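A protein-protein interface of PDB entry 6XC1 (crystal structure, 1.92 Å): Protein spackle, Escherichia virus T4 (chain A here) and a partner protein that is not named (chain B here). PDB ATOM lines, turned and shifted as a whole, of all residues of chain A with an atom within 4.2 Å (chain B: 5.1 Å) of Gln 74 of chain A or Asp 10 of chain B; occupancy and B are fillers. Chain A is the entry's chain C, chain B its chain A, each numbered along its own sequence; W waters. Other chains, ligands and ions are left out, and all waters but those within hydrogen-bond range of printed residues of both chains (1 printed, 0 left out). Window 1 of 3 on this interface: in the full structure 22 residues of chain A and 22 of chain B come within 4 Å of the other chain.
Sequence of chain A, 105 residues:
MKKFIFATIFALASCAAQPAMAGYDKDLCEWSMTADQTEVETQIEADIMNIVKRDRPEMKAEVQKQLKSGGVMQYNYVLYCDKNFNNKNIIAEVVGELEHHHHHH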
ATOM      1  N   GLY A  70     -10.556   5.765   0.890  1.00  0.00           N
ATOM      2  CA  GLY A  70     -11.596   5.292   1.786  1.00  0.00           C
ATOM      3  C   GLY A  70     -12.751   4.544   1.142  1.00  0.00           C
ATOM      4  O   GLY A  70     -13.577   3.954   1.847  1.00  0.00           O
ATOM      5  N   GLY A  71     -12.833   4.556  -0.183  1.00  0.00           N
ATOM      6  CA  GLY A  71     -13.900   3.874  -0.884  1.00  0.00           C
ATOM      7  C   GLY A  71     -15.054   4.805  -1.216  1.00  0.00           C
ATOM      8  O   GLY A  71     -15.143   5.942  -0.743  1.00  0.00           O
ATOM      9  N   VAL A  72     -15.949   4.316  -2.072  1.00  0.00           N
ATOM     10  CA  VAL A  72     -17.113   5.103  -2.463  1.00  0.00           C
ATOM     11  C   VAL A  72     -18.437   4.369  -2.270  1.00  0.00           C
ATOM     12  O   VAL A  72     -19.473   5.034  -2.116  1.00  0.00           O
ATOM     13  CB  VAL A  72     -16.983   5.627  -3.918  1.00  0.00           C
ATOM     14  CG1 VAL A  72     -15.628   5.277  -4.522  1.00  0.00           C
ATOM     15  CG2 VAL A  72     -18.123   5.164  -4.816  1.00  0.00           C
ATOM     16  N   MET A  73     -18.457   3.036  -2.208  1.00  0.00           N
ATOM     17  CA  MET A  73     -19.735   2.325  -2.149  1.00  0.00           C
ATOM     18  C   MET A  73     -20.530   2.669  -0.894  1.00  0.00           C
ATOM     19  O   MET A  73     -21.767   2.682  -0.926  1.00  0.00           O
ATOM     20  CB  MET A  73     -19.508   0.816  -2.221  1.00  0.00           C
ATOM     21  CG  MET A  73     -20.790   0.003  -2.143  1.00  0.00           C
ATOM     22  SD  MET A  73     -21.926   0.360  -3.509  1.00  0.00           S
ATOM     23  CE  MET A  73     -21.055  -0.430  -4.862  1.00  0.00           C
ATOM     24  N   GLN A  74     -19.845   2.971   0.211  1.00  0.00           N
ATOM     25  CA  GLN A  74     -20.525   3.103   1.497  1.00  0.00           C
ATOM     26  C   GLN A  74     -21.504   4.266   1.537  1.00  0.00           C
ATOM     27  O   GLN A  74     -22.363   4.298   2.424  1.00  0.00           O
ATOM     28  CB  GLN A  74     -19.507   3.265   2.626  1.00  0.00           C
ATOM     29  CG  GLN A  74     -18.640   4.522   2.515  1.00  0.00           C
ATOM     30  CD  GLN A  74     -17.270   4.225   1.943  1.00  0.00           C
ATOM     31  OE1 GLN A  74     -17.133   3.425   1.019  1.00  0.00           O
ATOM     32  NE2 GLN A  74     -16.243   4.863   2.498  1.00  0.00           N
ATOM     33  N   TYR A  75     -21.406   5.211   0.606  1.00  0.00           N
ATOM     34  CA  TYR A  75     -22.277   6.377   0.643  1.00  0.00           C
ATOM     35  C   TYR A  75     -23.621   6.135  -0.029  1.00  0.00           C
ATOM     36  O   TYR A  75     -24.432   7.064  -0.102  1.00  0.00           O
ATOM     37  CB  TYR A  75     -21.566   7.574  -0.003  1.00  0.00           C
ATOM     38  CG  TYR A  75     -20.224   7.847   0.644  1.00  0.00           C
ATOM     39  CD1 TYR A  75     -20.148   8.380   1.927  1.00  0.00           C
ATOM     40  CD2 TYR A  75     -19.036   7.551  -0.015  1.00  0.00           C
ATOM     41  CE1 TYR A  75     -18.922   8.621   2.536  1.00  0.00           C
ATOM     42  CE2 TYR A  75     -17.801   7.794   0.583  1.00  0.00           C
ATOM     43  CZ  TYR A  75     -17.751   8.323   1.859  1.00  0.00           C
ATOM     44  OH  TYR A  75     -16.525   8.567   2.460  1.00  0.00           O
ATOM     45  N   ASN A  76     -23.884   4.915  -0.510  1.00  0.00           N
ATOM     46  CA  ASN A  76     -25.127   4.682  -1.233  1.00  0.00           C
ATOM     47  C   ASN A  76     -26.337   4.901  -0.331  1.00  0.00           C
ATOM     48  O   ASN A  76     -27.358   5.436  -0.777  1.00  0.00           O
ATOM     49  CB  ASN A  76     -25.132   3.278  -1.854  1.00  0.00           C
ATOM     50  CG  ASN A  76     -25.500   2.184  -0.865  1.00  0.00           C
ATOM     51  OD1 ASN A  76     -24.908   2.063   0.205  1.00  0.00           O
ATOM     52  ND2 ASN A  76     -26.488   1.370  -1.231  1.00  0.00           N
ATOM     53  N   TYR A  77     -26.231   4.541   0.950  1.00  0.00           N
ATOM     54  CA  TYR A  77     -27.394   4.643   1.826  1.00  0.00           C
ATOM     55  C   TYR A  77     -27.761   6.099   2.099  1.00  0.00           C
ATOM     56  O   TYR A  77     -28.927   6.483   1.972  1.00  0.00           O
ATOM     57  CB  TYR A  77     -27.167   3.893   3.143  1.00  0.00           C
ATOM     58  CG  TYR A  77     -28.436   3.884   3.963  1.00  0.00           C
ATOM     59  CD1 TYR A  77     -29.404   2.908   3.762  1.00  0.00           C
ATOM     60  CD2 TYR A  77     -28.697   4.885   4.894  1.00  0.00           C
ATOM     61  CE1 TYR A  77     -30.586   2.914   4.479  1.00  0.00           C
ATOM     62  CE2 TYR A  77     -29.875   4.897   5.619  1.00  0.00           C
ATOM     63  CZ  TYR A  77     -30.815   3.908   5.406  1.00  0.00           C
ATOM     64  OH  TYR A  77     -31.990   3.911   6.120  1.00  0.00           O
ATOM     65  N   MET B   6     -26.170   3.812  12.933  1.00  0.00           N
ATOM     66  CA  MET B   6     -24.832   4.390  12.819  1.00  0.00           C
ATOM     67  C   MET B   6     -24.003   3.661  11.764  1.00  0.00           C
ATOM     68  O   MET B   6     -23.367   4.290  10.909  1.00  0.00           O
ATOM     69  CB  MET B   6     -24.138   4.339  14.182  1.00  0.00           C
ATOM     70  CG  MET B   6     -22.775   5.022  14.266  1.00  0.00           C
ATOM     71  SD  MET B   6     -21.931   4.546  15.792  1.00  0.00           S
ATOM     72  CE  MET B   6     -20.785   5.899  16.027  1.00  0.00           C
ATOM     73  N   LEU B   7     -23.998   2.326  11.809  1.00  0.00           N
ATOM     74  CA  LEU B   7     -23.151   1.564  10.900  1.00  0.00           C
ATOM     75  C   LEU B   7     -23.752   1.452   9.505  1.00  0.00           C
ATOM     76  O   LEU B   7     -23.008   1.322   8.527  1.00  0.00           O
ATOM     77  CB  LEU B   7     -22.878   0.178  11.480  1.00  0.00           C
ATOM     78  CG  LEU B   7     -21.928   0.207  12.684  1.00  0.00           C
ATOM     79  CD1 LEU B   7     -21.943  -1.122  13.433  1.00  0.00           C
ATOM     80  CD2 LEU B   7     -20.520   0.553  12.219  1.00  0.00           C
ATOM     81  N   ARG B   8     -25.080   1.500   9.391  1.00  0.00           N
ATOM     82  CA  ARG B   8     -25.699   1.601   8.072  1.00  0.00           C
ATOM     83  C   ARG B   8     -25.251   2.876   7.368  1.00  0.00           C
ATOM     84  O   ARG B   8     -24.930   2.865   6.175  1.00  0.00           O
ATOM     85  CB  ARG B   8     -27.219   1.567   8.211  1.00  0.00           C
ATOM     86  CG  ARG B   8     -27.978   1.205   6.952  1.00  0.00           C
ATOM     87  CD  ARG B   8     -29.447   1.026   7.281  1.00  0.00           C
ATOM     88  NE  ARG B   8     -29.964   2.196   7.982  1.00  0.00           N
ATOM     89  CZ  ARG B   8     -31.169   2.266   8.535  1.00  0.00           C
ATOM     90  NH1 ARG B   8     -31.990   1.228   8.467  1.00  0.00           N
ATOM     91  NH2 ARG B   8     -31.552   3.376   9.152  1.00  0.00           N
ATOM     92  N   ARG B   9     -25.215   3.985   8.105  1.00  0.00           N
ATOM     93  CA  ARG B   9     -24.744   5.243   7.534  1.00  0.00           C
ATOM     94  C   ARG B   9     -23.287   5.136   7.105  1.00  0.00           C
ATOM     95  O   ARG B   9     -22.933   5.493   5.975  1.00  0.00           O
ATOM     96  CB  ARG B   9     -24.933   6.373   8.548  1.00  0.00           C
ATOM     97  CG  ARG B   9     -24.283   7.687   8.150  1.00  0.00           C
ATOM     98  CD  ARG B   9     -24.642   8.783   9.130  1.00  0.00           C
ATOM     99  NE  ARG B   9     -23.960  10.038   8.829  1.00  0.00           N
ATOM    100  CZ  ARG B   9     -24.249  11.198   9.410  1.00  0.00           C
ATOM    101  NH1 ARG B   9     -25.216  11.266  10.316  1.00  0.00           N
ATOM    102  NH2 ARG B   9     -23.575  12.292   9.085  1.00  0.00           N
ATOM    103  N   ASP B  10     -22.430   4.616   7.989  1.00  0.00           N
ATOM    104  CA  ASP B  10     -20.995   4.628   7.734  1.00  0.00           C
ATOM    105  C   ASP B  10     -20.555   3.552   6.744  1.00  0.00           C
ATOM    106  O   ASP B  10     -19.568   3.753   6.030  1.00  0.00           O
ATOM    107  CB  ASP B  10     -20.225   4.477   9.050  1.00  0.00           C
ATOM    108  CG  ASP B  10     -20.200   5.766   9.874  1.00  0.00           C
ATOM    109  OD1 ASP B  10     -20.460   6.856   9.314  1.00  0.00           O
ATOM    110  OD2 ASP B  10     -19.894   5.689  11.085  1.00  0.00           O
ATOM    111  N   GLU B  11     -21.263   2.418   6.676  1.00  0.00           N
ATOM    112  CA  GLU B  11     -20.860   1.275   5.860  1.00  0.00           C
ATOM    113  C   GLU B  11     -21.673   1.102   4.584  1.00  0.00           C
ATOM    114  O   GLU B  11     -21.270   0.314   3.719  1.00  0.00           O
ATOM    115  CB  GLU B  11     -20.966  -0.036   6.670  1.00  0.00           C
ATOM    116  CG  GLU B  11     -20.115  -0.110   7.936  1.00  0.00           C
ATOM    117  CD  GLU B  11     -18.665  -0.452   7.651  1.00  0.00           C
ATOM    118  OE1 GLU B  11     -17.831  -0.366   8.579  1.00  0.00           O
ATOM    119  OE2 GLU B  11     -18.358  -0.804   6.493  1.00  0.00           O
ATOM    120  N   GLY B  12     -22.797   1.791   4.446  1.00  0.00           N
ATOM    121  CA  GLY B  12     -23.651   1.589   3.301  1.00  0.00           C
ATOM    122  C   GLY B  12     -24.479   0.326   3.453  1.00  0.00           C
ATOM    123  O   GLY B  12     -24.469  -0.343   4.490  1.00  0.00           O
ATOM    124  N   ASN B 106     -17.771   1.375  16.680  1.00  0.00           N
ATOM    125  CA  ASN B 106     -17.703   1.757  15.272  1.00  0.00           C
ATOM    126  C   ASN B 106     -16.318   1.478  14.703  1.00  0.00           C
ATOM    127  O   ASN B 106     -16.182   0.878  13.628  1.00  0.00           O
ATOM    128  CB  ASN B 106     -18.065   3.233  15.110  1.00  0.00           C
ATOM    129  CG  ASN B 106     -18.169   3.657  13.653  1.00  0.00           C
ATOM    130  OD1 ASN B 106     -17.189   3.620  12.910  1.00  0.00           O
ATOM    131  ND2 ASN B 106     -19.364   4.069  13.242  1.00  0.00           N
ATOM    132  N   ARG B 150     -15.500   9.558   8.167  1.00  0.00           N
ATOM    133  CA  ARG B 150     -15.910   8.686   9.262  1.00  0.00           C
ATOM    134  C   ARG B 150     -15.071   8.925  10.511  1.00  0.00           C
ATOM    135  O   ARG B 150     -15.608   8.968  11.623  1.00  0.00           O
ATOM    136  CB  ARG B 150     -15.813   7.231   8.816  1.00  0.00           C
ATOM    137  CG  ARG B 150     -16.255   6.219   9.862  1.00  0.00           C
ATOM    138  CD  ARG B 150     -16.377   4.852   9.213  1.00  0.00           C
ATOM    139  NE  ARG B 150     -16.799   3.815  10.150  1.00  0.00           N
ATOM    140  CZ  ARG B 150     -16.985   2.545   9.803  1.00  0.00           C
ATOM    141  NH1 ARG B 150     -17.371   1.651  10.702  1.00  0.00           N
ATOM    142  NH2 ARG B 150     -16.781   2.173   8.547  1.00  0.00           N
ATOM    143  N   ARG B 153     -16.230  12.017  12.367  1.00  0.00           N
ATOM    144  CA  ARG B 153     -17.440  11.755  13.142  1.00  0.00           C
ATOM    145  C   ARG B 153     -17.121  10.987  14.414  1.00  0.00           C
ATOM    146  O   ARG B 153     -17.638  11.307  15.491  1.00  0.00           O
ATOM    147  CB  ARG B 153     -18.448  10.961  12.304  1.00  0.00           C
ATOM    148  CG  ARG B 153     -19.014  11.695  11.117  1.00  0.00           C
ATOM    149  CD  ARG B 153     -20.219  10.965  10.523  1.00  0.00           C
ATOM    150  NE  ARG B 153     -19.858   9.789   9.730  1.00  0.00           N
ATOM    151  CZ  ARG B 153     -19.305   9.835   8.521  1.00  0.00           C
ATOM    152  NH1 ARG B 153     -19.026  11.005   7.959  1.00  0.00           N
ATOM    153  NH2 ARG B 153     -19.028   8.708   7.870  1.00  0.00           N
ATOM    154  N   VAL B 154     -16.269   9.967  14.310  1.00  0.00           N
ATOM    155  CA  VAL B 154     -16.005   9.099  15.452  1.00  0.00           C
ATOM    156  C   VAL B 154     -15.173   9.824  16.507  1.00  0.00           C
ATOM    157  O   VAL B 154     -15.477   9.756  17.704  1.00  0.00           O
ATOM    158  CB  VAL B 154     -15.332   7.799  14.978  1.00  0.00           C
ATOM    159  CG1 VAL B 154     -14.891   6.963  16.167  1.00  0.00           C
ATOM    160  CG2 VAL B 154     -16.291   7.008  14.075  1.00  0.00           C
ATOM    161  N   TYR B 166     -23.303  12.538  14.603  1.00  0.00           N
ATOM    162  CA  TYR B 166     -24.172  11.716  13.772  1.00  0.00           C
ATOM    163  C   TYR B 166     -25.586  12.282  13.680  1.00  0.00           C
ATOM    164  O   TYR B 166     -26.517  11.556  13.319  1.00  0.00           O
ATOM    165  CB  TYR B 166     -24.201  10.279  14.294  1.00  0.00           C
ATOM    166  CG  TYR B 166     -22.985   9.490  13.873  1.00  0.00           C
ATOM    167  CD1 TYR B 166     -21.807   9.557  14.604  1.00  0.00           C
ATOM    168  CD2 TYR B 166     -23.003   8.706  12.727  1.00  0.00           C
ATOM    169  CE1 TYR B 166     -20.685   8.858  14.210  1.00  0.00           C
ATOM    170  CE2 TYR B 166     -21.887   7.995  12.332  1.00  0.00           C
ATOM    171  CZ  TYR B 166     -20.727   8.080  13.080  1.00  0.00           C
ATOM    172  OH  TYR B 166     -19.607   7.382  12.694  1.00  0.00           O
HETATM  173  O   HOH W   1     -24.381   5.750   3.617  1.00  0.00           O
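O of Gln 74 of chain A lies close to N of Gly 12 of chain B (3.2 Å).
The guanidinium group (NH2) of Arg 8 of chain B lies close to the side-chain hydroxyl (OH) of Tyr 77 of chain A, 3.1 Å away.
Water W1 lies within hydrogen-bond range of O of Gln 74 of chain A (2.8 Å), O of Arg 9 of chain B (2.8 Å) and N of Tyr 77 of chain A (3.5 Å).
The backbone carbonyl oxygen (O) of Met 73 of chain A sits close to the side-chain amide oxygen (OD1) of Asn 76 of chain A (3.4 Å).
NE of Arg 150 of chain B lies within salt-bridge range of OD2 of Asp 10 of chain B (3.7 Å).
The backbone carbonyl oxygen of Tyr 166 of chain B lies within hydrogen-bond range of the guanidinium group of Arg 9 of chain B, 3.3 Å away.
The guanidinium group (NH2) of Arg 150 of chain B lies within salt-bridge range of the side-chain carboxylate (OE1) of Glu 11 of chain B, at 2.7 Å.
The side-chain carboxylate (OD2) of Asp 10 of chain B sits at hydrogen-bond distance from the side-chain amide nitrogen (ND2) of Asn 106 of chain B (2.7 Å).
NH2 of Arg 153 of chain B lies within salt-bridge range of OD1 of Asp 10 of chain B (2.8 Å).
Of chain B, only Arg 9, Asp 10, Glu 11 and Gly 12 come within 4 Å of Gln 74 of chain A.
Of the printed residues of chain B, Asn 76 of chain A touches Gly 12 (3.4 Å).
Of the printed residues of chain A, Arg 8 of chain B touches Tyr 77.
Printed residues of chain A within 4 Å of Arg 9 of chain B: Gln 74.
Of chain A, only Gln 74 (3.4 Å) comes within 4 Å of Asp 10 of chain B.
The nearest residue of chain B that does not touch Gln 74 of chain A is Arg 8 of chain B (4.8 Å).
Gln 74 of chain A touches Arg 9 of chain B.
Asp 10 of chain B touches Gln 74 of chain A (O to CB, 3.4 Å).
Gln 74 of chain A touches Glu 11 of chain B.
OD1 of Asn 76 of chain A touches CA of Gly 12 of chain B, 3.4 Å away.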
